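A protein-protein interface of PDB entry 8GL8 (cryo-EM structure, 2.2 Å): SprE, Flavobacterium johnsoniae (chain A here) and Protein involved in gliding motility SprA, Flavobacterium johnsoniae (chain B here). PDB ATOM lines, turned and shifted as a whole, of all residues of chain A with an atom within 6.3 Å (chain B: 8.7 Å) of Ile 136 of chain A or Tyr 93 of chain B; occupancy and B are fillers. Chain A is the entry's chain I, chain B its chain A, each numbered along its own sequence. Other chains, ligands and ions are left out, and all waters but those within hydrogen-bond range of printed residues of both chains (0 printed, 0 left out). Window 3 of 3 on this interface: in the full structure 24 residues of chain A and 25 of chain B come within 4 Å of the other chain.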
ATOM      1  N   ARG A 129     -29.531 -11.356 -15.126  1.00  0.00           N
ATOM      2  CA  ARG A 129     -28.810 -10.505 -14.184  1.00  0.00           C
ATOM      3  C   ARG A 129     -27.373 -10.274 -14.634  1.00  0.00           C
ATOM      4  O   ARG A 129     -26.830  -9.178 -14.456  1.00  0.00           O
ATOM      5  CB  ARG A 129     -28.846 -11.119 -12.788  1.00  0.00           C
ATOM      6  CG  ARG A 129     -30.216 -11.098 -12.150  1.00  0.00           C
ATOM      7  CD  ARG A 129     -30.257 -11.951 -10.904  1.00  0.00           C
ATOM      8  NE  ARG A 129     -31.375 -11.592 -10.042  1.00  0.00           N
ATOM      9  CZ  ARG A 129     -31.706 -12.242  -8.936  1.00  0.00           C
ATOM     10  NH1 ARG A 129     -31.013 -13.285  -8.514  1.00  0.00           N
ATOM     11  NH2 ARG A 129     -32.761 -11.836  -8.237  1.00  0.00           N
ATOM     12  N   ARG A 134     -25.416  -7.052 -13.087  1.00  0.00           N
ATOM     13  CA  ARG A 134     -25.658  -7.233 -11.658  1.00  0.00           C
ATOM     14  C   ARG A 134     -25.091  -8.603 -11.305  1.00  0.00           C
ATOM     15  O   ARG A 134     -25.796  -9.611 -11.333  1.00  0.00           O
ATOM     16  CB  ARG A 134     -27.141  -7.129 -11.329  1.00  0.00           C
ATOM     17  CG  ARG A 134     -27.884  -6.104 -12.159  1.00  0.00           C
ATOM     18  CD  ARG A 134     -28.979  -5.435 -11.352  1.00  0.00           C
ATOM     19  NE  ARG A 134     -29.786  -6.403 -10.619  1.00  0.00           N
ATOM     20  CZ  ARG A 134     -30.795  -7.085 -11.139  1.00  0.00           C
ATOM     21  NH1 ARG A 134     -31.154  -6.932 -12.402  1.00  0.00           N
ATOM     22  NH2 ARG A 134     -31.461  -7.943 -10.372  1.00  0.00           N
ATOM     23  N   PHE A 135     -23.804  -8.631 -10.965  1.00  0.00           N
ATOM     24  CA  PHE A 135     -23.079  -9.893 -10.928  1.00  0.00           C
ATOM     25  C   PHE A 135     -23.285 -10.667  -9.633  1.00  0.00           C
ATOM     26  O   PHE A 135     -23.260 -11.899  -9.654  1.00  0.00           O
ATOM     27  CB  PHE A 135     -21.594  -9.636 -11.173  1.00  0.00           C
ATOM     28  CG  PHE A 135     -21.313  -9.004 -12.502  1.00  0.00           C
ATOM     29  CD1 PHE A 135     -21.770  -9.589 -13.668  1.00  0.00           C
ATOM     30  CD2 PHE A 135     -20.613  -7.817 -12.585  1.00  0.00           C
ATOM     31  CE1 PHE A 135     -21.523  -9.009 -14.892  1.00  0.00           C
ATOM     32  CE2 PHE A 135     -20.363  -7.233 -13.808  1.00  0.00           C
ATOM     33  CZ  PHE A 135     -20.818  -7.831 -14.961  1.00  0.00           C
ATOM     34  N   ILE A 136     -23.484  -9.991  -8.507  1.00  0.00           N
ATOM     35  CA  ILE A 136     -23.699 -10.703  -7.247  1.00  0.00           C
ATOM     36  C   ILE A 136     -25.020 -11.472  -7.284  1.00  0.00           C
ATOM     37  O   ILE A 136     -25.029 -12.664  -6.943  1.00  0.00           O
ATOM     38  CB  ILE A 136     -23.623  -9.748  -6.044  1.00  0.00           C
ATOM     39  CG1 ILE A 136     -22.273  -9.028  -6.021  1.00  0.00           C
ATOM     40  CG2 ILE A 136     -23.860 -10.504  -4.747  1.00  0.00           C
ATOM     41  CD1 ILE A 136     -21.193  -9.765  -5.265  1.00  0.00           C
ATOM     42  N   PRO A 137     -26.153 -10.867  -7.669  1.00  0.00           N
ATOM     43  CA  PRO A 137     -27.381 -11.674  -7.797  1.00  0.00           C
ATOM     44  C   PRO A 137     -27.302 -12.753  -8.868  1.00  0.00           C
ATOM     45  O   PRO A 137     -27.899 -13.825  -8.699  1.00  0.00           O
ATOM     46  CB  PRO A 137     -28.460 -10.630  -8.120  1.00  0.00           C
ATOM     47  CG  PRO A 137     -27.733  -9.425  -8.550  1.00  0.00           C
ATOM     48  CD  PRO A 137     -26.444  -9.431  -7.824  1.00  0.00           C
ATOM     49  N   ALA A 138     -26.586 -12.508  -9.968  1.00  0.00           N
ATOM     50  CA  ALA A 138     -26.409 -13.543 -10.982  1.00  0.00           C
ATOM     51  C   ALA A 138     -25.660 -14.739 -10.412  1.00  0.00           C
ATOM     52  O   ALA A 138     -26.050 -15.897 -10.617  1.00  0.00           O
ATOM     53  CB  ALA A 138     -25.670 -12.968 -12.188  1.00  0.00           C
ATOM     54  N   LEU A 139     -24.580 -14.469  -9.678  1.00  0.00           N
ATOM     55  CA  LEU A 139     -23.843 -15.530  -9.007  1.00  0.00           C
ATOM     56  C   LEU A 139     -24.724 -16.250  -8.001  1.00  0.00           C
ATOM     57  O   LEU A 139     -24.622 -17.469  -7.842  1.00  0.00           O
ATOM     58  CB  LEU A 139     -22.609 -14.948  -8.322  1.00  0.00           C
ATOM     59  CG  LEU A 139     -21.606 -15.911  -7.688  1.00  0.00           C
ATOM     60  CD1 LEU A 139     -21.442 -17.155  -8.532  1.00  0.00           C
ATOM     61  CD2 LEU A 139     -20.277 -15.218  -7.507  1.00  0.00           C
ATOM     62  N   GLU A 140     -25.590 -15.510  -7.308  1.00  0.00           N
ATOM     63  CA  GLU A 140     -26.507 -16.143  -6.368  1.00  0.00           C
ATOM     64  C   GLU A 140     -27.440 -17.117  -7.074  1.00  0.00           C
ATOM     65  O   GLU A 140     -27.682 -18.223  -6.581  1.00  0.00           O
ATOM     66  CB  GLU A 140     -27.307 -15.080  -5.620  1.00  0.00           C
ATOM     67  CG  GLU A 140     -27.886 -15.565  -4.309  1.00  0.00           C
ATOM     68  CD  GLU A 140     -28.993 -14.675  -3.798  1.00  0.00           C
ATOM     69  OE1 GLU A 140     -29.349 -13.704  -4.499  1.00  0.00           O
ATOM     70  OE2 GLU A 140     -29.509 -14.943  -2.693  1.00  0.00           O
ATOM     71  N   ALA A 141     -27.971 -16.724  -8.233  1.00  0.00           N
ATOM     72  CA  ALA A 141     -28.850 -17.616  -8.986  1.00  0.00           C
ATOM     73  C   ALA A 141     -28.115 -18.868  -9.457  1.00  0.00           C
ATOM     74  O   ALA A 141     -28.634 -19.988  -9.339  1.00  0.00           O
ATOM     75  CB  ALA A 141     -29.457 -16.871 -10.173  1.00  0.00           C
ATOM     76  N   THR A 165     -19.203 -15.239 -14.060  1.00  0.00           N
ATOM     77  CA  THR A 165     -19.627 -14.228 -13.099  1.00  0.00           C
ATOM     78  C   THR A 165     -18.506 -13.899 -12.122  1.00  0.00           C
ATOM     79  O   THR A 165     -18.293 -12.730 -11.781  1.00  0.00           O
ATOM     80  CB  THR A 165     -20.870 -14.698 -12.349  1.00  0.00           C
ATOM     81  OG1 THR A 165     -21.869 -15.105 -13.288  1.00  0.00           O
ATOM     82  CG2 THR A 165     -21.418 -13.577 -11.514  1.00  0.00           C
ATOM     83  N   LEU A 169     -16.376 -10.429 -11.407  1.00  0.00           N
ATOM     84  CA  LEU A 169     -16.174  -9.907 -10.064  1.00  0.00           C
ATOM     85  C   LEU A 169     -14.703  -9.771  -9.693  1.00  0.00           C
ATOM     86  O   LEU A 169     -14.399  -9.329  -8.582  1.00  0.00           O
ATOM     87  CB  LEU A 169     -16.883 -10.801  -9.042  1.00  0.00           C
ATOM     88  CG  LEU A 169     -18.410 -10.776  -9.073  1.00  0.00           C
ATOM     89  CD1 LEU A 169     -18.981 -11.859  -8.183  1.00  0.00           C
ATOM     90  CD2 LEU A 169     -18.933  -9.415  -8.662  1.00  0.00           C
ATOM     91  N   LEU B  85     -14.206  -3.484   9.460  1.00  0.00           N
ATOM     92  CA  LEU B  85     -14.947  -3.142   8.251  1.00  0.00           C
ATOM     93  C   LEU B  85     -15.640  -4.364   7.667  1.00  0.00           C
ATOM     94  O   LEU B  85     -16.802  -4.288   7.259  1.00  0.00           O
ATOM     95  CB  LEU B  85     -14.008  -2.515   7.221  1.00  0.00           C
ATOM     96  CG  LEU B  85     -14.644  -2.133   5.886  1.00  0.00           C
ATOM     97  CD1 LEU B  85     -15.268  -0.753   5.971  1.00  0.00           C
ATOM     98  CD2 LEU B  85     -13.616  -2.192   4.770  1.00  0.00           C
ATOM     99  N   LEU B  86     -14.946  -5.504   7.627  1.00  0.00           N
ATOM    100  CA  LEU B  86     -15.551  -6.726   7.114  1.00  0.00           C
ATOM    101  C   LEU B  86     -16.701  -7.189   7.998  1.00  0.00           C
ATOM    102  O   LEU B  86     -17.742  -7.622   7.493  1.00  0.00           O
ATOM    103  CB  LEU B  86     -14.493  -7.821   6.989  1.00  0.00           C
ATOM    104  CG  LEU B  86     -13.862  -8.037   5.612  1.00  0.00           C
ATOM    105  CD1 LEU B  86     -13.556  -6.716   4.929  1.00  0.00           C
ATOM    106  CD2 LEU B  86     -12.606  -8.880   5.731  1.00  0.00           C
ATOM    107  N   LYS B  87     -16.532  -7.104   9.319  1.00  0.00           N
ATOM    108  CA  LYS B  87     -17.598  -7.499  10.234  1.00  0.00           C
ATOM    109  C   LYS B  87     -18.843  -6.644  10.030  1.00  0.00           C
ATOM    110  O   LYS B  87     -19.961  -7.164   9.903  1.00  0.00           O
ATOM    111  CB  LYS B  87     -17.100  -7.395  11.675  1.00  0.00           C
ATOM    112  CG  LYS B  87     -17.971  -8.095  12.698  1.00  0.00           C
ATOM    113  CD  LYS B  87     -17.743  -7.516  14.082  1.00  0.00           C
ATOM    114  CE  LYS B  87     -17.305  -8.588  15.064  1.00  0.00           C
ATOM    115  NZ  LYS B  87     -17.664  -8.237  16.465  1.00  0.00           N
ATOM    116  N   GLU B  88     -18.664  -5.323   9.979  1.00  0.00           N
ATOM    117  CA  GLU B  88     -19.811  -4.440   9.807  1.00  0.00           C
ATOM    118  C   GLU B  88     -20.424  -4.579   8.420  1.00  0.00           C
ATOM    119  O   GLU B  88     -21.643  -4.459   8.274  1.00  0.00           O
ATOM    120  CB  GLU B  88     -19.413  -2.990  10.093  1.00  0.00           C
ATOM    121  CG  GLU B  88     -18.601  -2.314   9.007  1.00  0.00           C
ATOM    122  CD  GLU B  88     -19.360  -1.194   8.326  1.00  0.00           C
ATOM    123  OE1 GLU B  88     -18.863  -0.669   7.307  1.00  0.00           O
ATOM    124  OE2 GLU B  88     -20.455  -0.836   8.812  1.00  0.00           O
ATOM    125  N   SER B  89     -19.613  -4.859   7.396  1.00  0.00           N
ATOM    126  CA  SER B  89     -20.158  -5.061   6.058  1.00  0.00           C
ATOM    127  C   SER B  89     -20.970  -6.346   5.980  1.00  0.00           C
ATOM    128  O   SER B  89     -22.025  -6.376   5.342  1.00  0.00           O
ATOM    129  CB  SER B  89     -19.031  -5.071   5.029  1.00  0.00           C
ATOM    130  OG  SER B  89     -18.482  -6.368   4.889  1.00  0.00           O
ATOM    131  N   ARG B  90     -20.498  -7.416   6.623  1.00  0.00           N
ATOM    132  CA  ARG B  90     -21.274  -8.652   6.670  1.00  0.00           C
ATOM    133  C   ARG B  90     -22.594  -8.437   7.398  1.00  0.00           C
ATOM    134  O   ARG B  90     -23.655  -8.884   6.940  1.00  0.00           O
ATOM    135  CB  ARG B  90     -20.463  -9.753   7.350  1.00  0.00           C
ATOM    136  CG  ARG B  90     -19.312 -10.289   6.522  1.00  0.00           C
ATOM    137  CD  ARG B  90     -18.891 -11.664   7.000  1.00  0.00           C
ATOM    138  NE  ARG B  90     -18.339 -11.625   8.347  1.00  0.00           N
ATOM    139  CZ  ARG B  90     -17.076 -11.338   8.631  1.00  0.00           C
ATOM    140  NH1 ARG B  90     -16.200 -11.067   7.678  1.00  0.00           N
ATOM    141  NH2 ARG B  90     -16.683 -11.324   9.900  1.00  0.00           N
ATOM    142  N   ARG B  91     -22.545  -7.741   8.537  1.00  0.00           N
ATOM    143  CA  ARG B  91     -23.768  -7.474   9.286  1.00  0.00           C
ATOM    144  C   ARG B  91     -24.740  -6.632   8.468  1.00  0.00           C
ATOM    145  O   ARG B  91     -25.944  -6.909   8.445  1.00  0.00           O
ATOM    146  CB  ARG B  91     -23.430  -6.785  10.607  1.00  0.00           C
ATOM    147  CG  ARG B  91     -24.584  -6.030  11.236  1.00  0.00           C
ATOM    148  CD  ARG B  91     -24.140  -5.288  12.482  1.00  0.00           C
ATOM    149  NE  ARG B  91     -23.174  -6.053  13.261  1.00  0.00           N
ATOM    150  CZ  ARG B  91     -21.989  -5.596  13.642  1.00  0.00           C
ATOM    151  NH1 ARG B  91     -21.584  -4.378  13.325  1.00  0.00           N
ATOM    152  NH2 ARG B  91     -21.191  -6.382  14.358  1.00  0.00           N
ATOM    153  N   ASP B  92     -24.232  -5.609   7.778  1.00  0.00           N
ATOM    154  CA  ASP B  92     -25.089  -4.751   6.967  1.00  0.00           C
ATOM    155  C   ASP B  92     -25.680  -5.509   5.787  1.00  0.00           C
ATOM    156  O   ASP B  92     -26.843  -5.298   5.431  1.00  0.00           O
ATOM    157  CB  ASP B  92     -24.301  -3.536   6.484  1.00  0.00           C
ATOM    158  CG  ASP B  92     -24.422  -2.355   7.422  1.00  0.00           C
ATOM    159  OD1 ASP B  92     -25.338  -2.360   8.269  1.00  0.00           O
ATOM    160  OD2 ASP B  92     -23.599  -1.422   7.315  1.00  0.00           O
ATOM    161  N   TYR B  93     -24.894  -6.388   5.161  1.00  0.00           N
ATOM    162  CA  TYR B  93     -25.403  -7.188   4.052  1.00  0.00           C
ATOM    163  C   TYR B  93     -26.537  -8.094   4.511  1.00  0.00           C
ATOM    164  O   TYR B  93     -27.599  -8.153   3.876  1.00  0.00           O
ATOM    165  CB  TYR B  93     -24.265  -8.008   3.447  1.00  0.00           C
ATOM    166  CG  TYR B  93     -24.608  -8.692   2.147  1.00  0.00           C
ATOM    167  CD1 TYR B  93     -24.730  -7.967   0.972  1.00  0.00           C
ATOM    168  CD2 TYR B  93     -24.801 -10.063   2.094  1.00  0.00           C
ATOM    169  CE1 TYR B  93     -25.040  -8.590  -0.218  1.00  0.00           C
ATOM    170  CE2 TYR B  93     -25.109 -10.693   0.911  1.00  0.00           C
ATOM    171  CZ  TYR B  93     -25.227  -9.953  -0.243  1.00  0.00           C
ATOM    172  OH  TYR B  93     -25.535 -10.577  -1.427  1.00  0.00           O
ATOM    173  N   PHE B  94     -26.336  -8.796   5.630  1.00  0.00           N
ATOM    174  CA  PHE B  94     -27.399  -9.646   6.154  1.00  0.00           C
ATOM    175  C   PHE B  94     -28.633  -8.826   6.510  1.00  0.00           C
ATOM    176  O   PHE B  94     -29.763  -9.213   6.181  1.00  0.00           O
ATOM    177  CB  PHE B  94     -26.902 -10.421   7.373  1.00  0.00           C
ATOM    178  CG  PHE B  94     -26.115 -11.652   7.031  1.00  0.00           C
ATOM    179  CD1 PHE B  94     -26.494 -12.463   5.977  1.00  0.00           C
ATOM    180  CD2 PHE B  94     -24.997 -12.001   7.768  1.00  0.00           C
ATOM    181  CE1 PHE B  94     -25.772 -13.595   5.663  1.00  0.00           C
ATOM    182  CE2 PHE B  94     -24.273 -13.132   7.459  1.00  0.00           C
ATOM    183  CZ  PHE B  94     -24.661 -13.930   6.405  1.00  0.00           C
ATOM    184  N   ARG B  95     -28.435  -7.684   7.173  1.00  0.00           N
ATOM    185  CA  ARG B  95     -29.564  -6.861   7.588  1.00  0.00           C
ATOM    186  C   ARG B  95     -30.347  -6.351   6.388  1.00  0.00           C
ATOM    187  O   ARG B  95     -31.580  -6.372   6.391  1.00  0.00           O
ATOM    188  CB  ARG B  95     -29.071  -5.695   8.444  1.00  0.00           C
ATOM    189  CG  ARG B  95     -30.144  -4.681   8.792  1.00  0.00           C
ATOM    190  CD  ARG B  95     -30.050  -4.263  10.247  1.00  0.00           C
ATOM    191  NE  ARG B  95     -29.545  -5.340  11.090  1.00  0.00           N
ATOM    192  CZ  ARG B  95     -28.537  -5.214  11.940  1.00  0.00           C
ATOM    193  NH1 ARG B  95     -27.893  -4.067  12.082  1.00  0.00           N
ATOM    194  NH2 ARG B  95     -28.163  -6.264  12.664  1.00  0.00           N
ATOM    195  N   LYS B  96     -29.647  -5.894   5.347  1.00  0.00           N
ATOM    196  CA  LYS B  96     -30.326  -5.417   4.148  1.00  0.00           C
ATOM    197  C   LYS B  96     -31.078  -6.544   3.454  1.00  0.00           C
ATOM    198  O   LYS B  96     -32.189  -6.338   2.953  1.00  0.00           O
ATOM    199  CB  LYS B  96     -29.318  -4.776   3.195  1.00  0.00           C
ATOM    200  CG  LYS B  96     -28.919  -3.362   3.579  1.00  0.00           C
ATOM    201  CD  LYS B  96     -27.959  -2.762   2.564  1.00  0.00           C
ATOM    202  CE  LYS B  96     -26.517  -2.880   3.033  1.00  0.00           C
ATOM    203  NZ  LYS B  96     -25.618  -3.396   1.965  1.00  0.00           N
ATOM    204  N   LYS B  97     -30.494  -7.743   3.419  1.00  0.00           N
ATOM    205  CA  LYS B  97     -31.173  -8.864   2.778  1.00  0.00           C
ATOM    206  C   LYS B  97     -32.474  -9.208   3.497  1.00  0.00           C
ATOM    207  O   LYS B  97     -33.523  -9.370   2.860  1.00  0.00           O
ATOM    208  CB  LYS B  97     -30.246 -10.076   2.723  1.00  0.00           C
ATOM    209  CG  LYS B  97     -30.885 -11.310   2.120  1.00  0.00           C
ATOM    210  CD  LYS B  97     -29.957 -12.501   2.217  1.00  0.00           C
ATOM    211  CE  LYS B  97     -28.689 -12.273   1.417  1.00  0.00           C
ATOM    212  NZ  LYS B  97     -28.810 -12.815   0.038  1.00  0.00           N
ATOM    213  N   MET B  98     -32.437  -9.309   4.829  1.00  0.00           N
ATOM    214  CA  MET B  98     -33.676  -9.641   5.531  1.00  0.00           C
ATOM    215  C   MET B  98     -34.651  -8.469   5.572  1.00  0.00           C
ATOM    216  O   MET B  98     -35.863  -8.686   5.675  1.00  0.00           O
ATOM    217  CB  MET B  98     -33.399 -10.156   6.942  1.00  0.00           C
ATOM    218  CG  MET B  98     -32.043 -10.775   7.130  1.00  0.00           C
ATOM    219  SD  MET B  98     -31.878 -11.594   8.716  1.00  0.00           S
ATOM    220  CE  MET B  98     -33.299 -12.683   8.672  1.00  0.00           C
ATOM    221  N   ASP B  99     -34.161  -7.231   5.485  1.00  0.00           N
ATOM    222  CA  ASP B  99     -35.068  -6.098   5.344  1.00  0.00           C
ATOM    223  C   ASP B  99     -35.803  -6.152   4.011  1.00  0.00           C
ATOM    224  O   ASP B  99     -37.003  -5.865   3.946  1.00  0.00           O
ATOM    225  CB  ASP B  99     -34.300  -4.786   5.482  1.00  0.00           C
ATOM    226  CG  ASP B  99     -33.922  -4.481   6.917  1.00  0.00           C
ATOM    227  OD1 ASP B  99     -34.415  -5.184   7.824  1.00  0.00           O
ATOM    228  OD2 ASP B  99     -33.131  -3.540   7.139  1.00  0.00           O
ATOM    229  N   ALA B 100     -35.095  -6.514   2.938  1.00  0.00           N
ATOM    230  CA  ALA B 100     -35.746  -6.694   1.645  1.00  0.00           C
ATOM    231  C   ALA B 100     -36.742  -7.845   1.687  1.00  0.00           C
ATOM    232  O   ALA B 100     -37.829  -7.755   1.107  1.00  0.00           O
ATOM    233  CB  ALA B 100     -34.700  -6.928   0.557  1.00  0.00           C
ATOM    234  N   ASP B 114     -32.839  -7.491  -6.389  1.00  0.00           N
ATOM    235  CA  ASP B 114     -31.613  -8.262  -6.241  1.00  0.00           C
ATOM    236  C   ASP B 114     -31.777  -9.459  -5.316  1.00  0.00           C
ATOM    237  O   ASP B 114     -30.775 -10.061  -4.918  1.00  0.00           O
ATOM    238  CB  ASP B 114     -30.486  -7.362  -5.733  1.00  0.00           C
ATOM    239  CG  ASP B 114     -30.108  -6.284  -6.728  1.00  0.00           C
ATOM    240  OD1 ASP B 114     -29.898  -6.613  -7.913  1.00  0.00           O
ATOM    241  OD2 ASP B 114     -30.020  -5.107  -6.326  1.00  0.00           O
ATOM    242  N   LEU B 115     -33.006  -9.811  -4.969  1.00  0.00           N
ATOM    243  CA  LEU B 115     -33.305 -10.946  -4.114  1.00  0.00           C
ATOM    244  C   LEU B 115     -33.578 -12.187  -4.954  1.00  0.00           C
ATOM    245  O   LEU B 115     -33.971 -12.104  -6.120  1.00  0.00           O
ATOM    246  CB  LEU B 115     -34.515 -10.642  -3.230  1.00  0.00           C
ATOM    247  CG  LEU B 115     -34.479 -11.030  -1.755  1.00  0.00           C
ATOM    248  CD1 LEU B 115     -33.294 -10.392  -1.057  1.00  0.00           C
ATOM    249  CD2 LEU B 115     -35.780 -10.615  -1.097  1.00  0.00           C
ATOM    250  N   LEU B 116     -33.358 -13.342  -4.350  1.00  0.00           N
ATOM    251  CA  LEU B 116     -33.788 -14.587  -4.967  1.00  0.00           C
ATOM    252  C   LEU B 116     -35.309 -14.663  -4.914  1.00  0.00           C
ATOM    253  O   LEU B 116     -35.892 -14.507  -3.836  1.00  0.00           O
ATOM    254  CB  LEU B 116     -33.168 -15.785  -4.253  1.00  0.00           C
ATOM    255  CG  LEU B 116     -32.522 -16.874  -5.112  1.00  0.00           C
ATOM    256  CD1 LEU B 116     -31.569 -16.277  -6.134  1.00  0.00           C
ATOM    257  CD2 LEU B 116     -31.803 -17.879  -4.235  1.00  0.00           C
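OE2 of Glu 140 of chain A is in salt-bridge range of NZ of Lys 97 of chain B.
OD1 of Asp 114 of chain B is in salt-bridge range of NE of Arg 134 of chain A (2.7 Å).
The backbone carbonyl oxygen (O) of Leu 115 of chain B lies within hydrogen-bond range of the guanidinium group (NH2) of Arg 129 of chain A, at 2.5 Å.
Printed residues of chain B that touch a printed residue of chain A: Tyr 93, Lys 97, Asp 114, Leu 115 and Leu 116.
Hydrophobic or aromatic side chains of chain B that line the printed part of chain A: Tyr 93 and Leu 116.
Along chain B the printed residues that touch a printed residue of chain A span positions 93 to 116.
Among the printed residues, 9 pairs touch across the chains.
Asp 114 of chain B touches Arg 129 of chain A.
CD1 of Leu 116 of chain B touches NH1 of Arg 129 of chain A, at 3.9 Å.
Ile 136 of chain A touches Tyr 93 of chain B (CG2 to OH, 3.7 Å).
Asp 114 of chain B touches Pro 137 of chain A.
OE1 of Glu 140 of chain A touches O of Asp 114 of chain B (3.9 Å).
Glu 140 of chain A touches Leu 116 of chain B (OE1 to CD1, 3.8 Å).
The backbone NH (N) of Arg 134 of chain A lies within hydrogen-bond range of the backbone carbonyl oxygen (O) of Arg 129 of chain A (2.9 Å).
The guanidinium group (NH1) of Arg 129 of chain A lies within hydrogen-bond range of the backbone carbonyl oxygen (O) of Pro 137 of chain A, 3.2 Å away.
Ile 136 of chain A touches just one residue of chain B: Tyr 93 (3.7 Å).
Tyr 93 of chain B touches just one residue of chain A: Ile 136.
Of the printed residues of chain B, Arg 134 of chain A touches Asp 114.
Of the printed residues of chain A, Leu 116 of chain B touches Arg 129 and Glu 140.
Printed residues of chain B within 4 Å of Glu 140 of chain A: Lys 97 (3.5 Å), Asp 114 (3.9 Å) and Leu 116 (3.8 Å).
The nearest residue of chain B that does not touch Ile 136 of chain A is Asp 114 of chain B (6.4 Å).
The nearest printed residue of chain B that does not touch Arg 134 of chain A is Leu 115 of chain B (5.9 Å).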
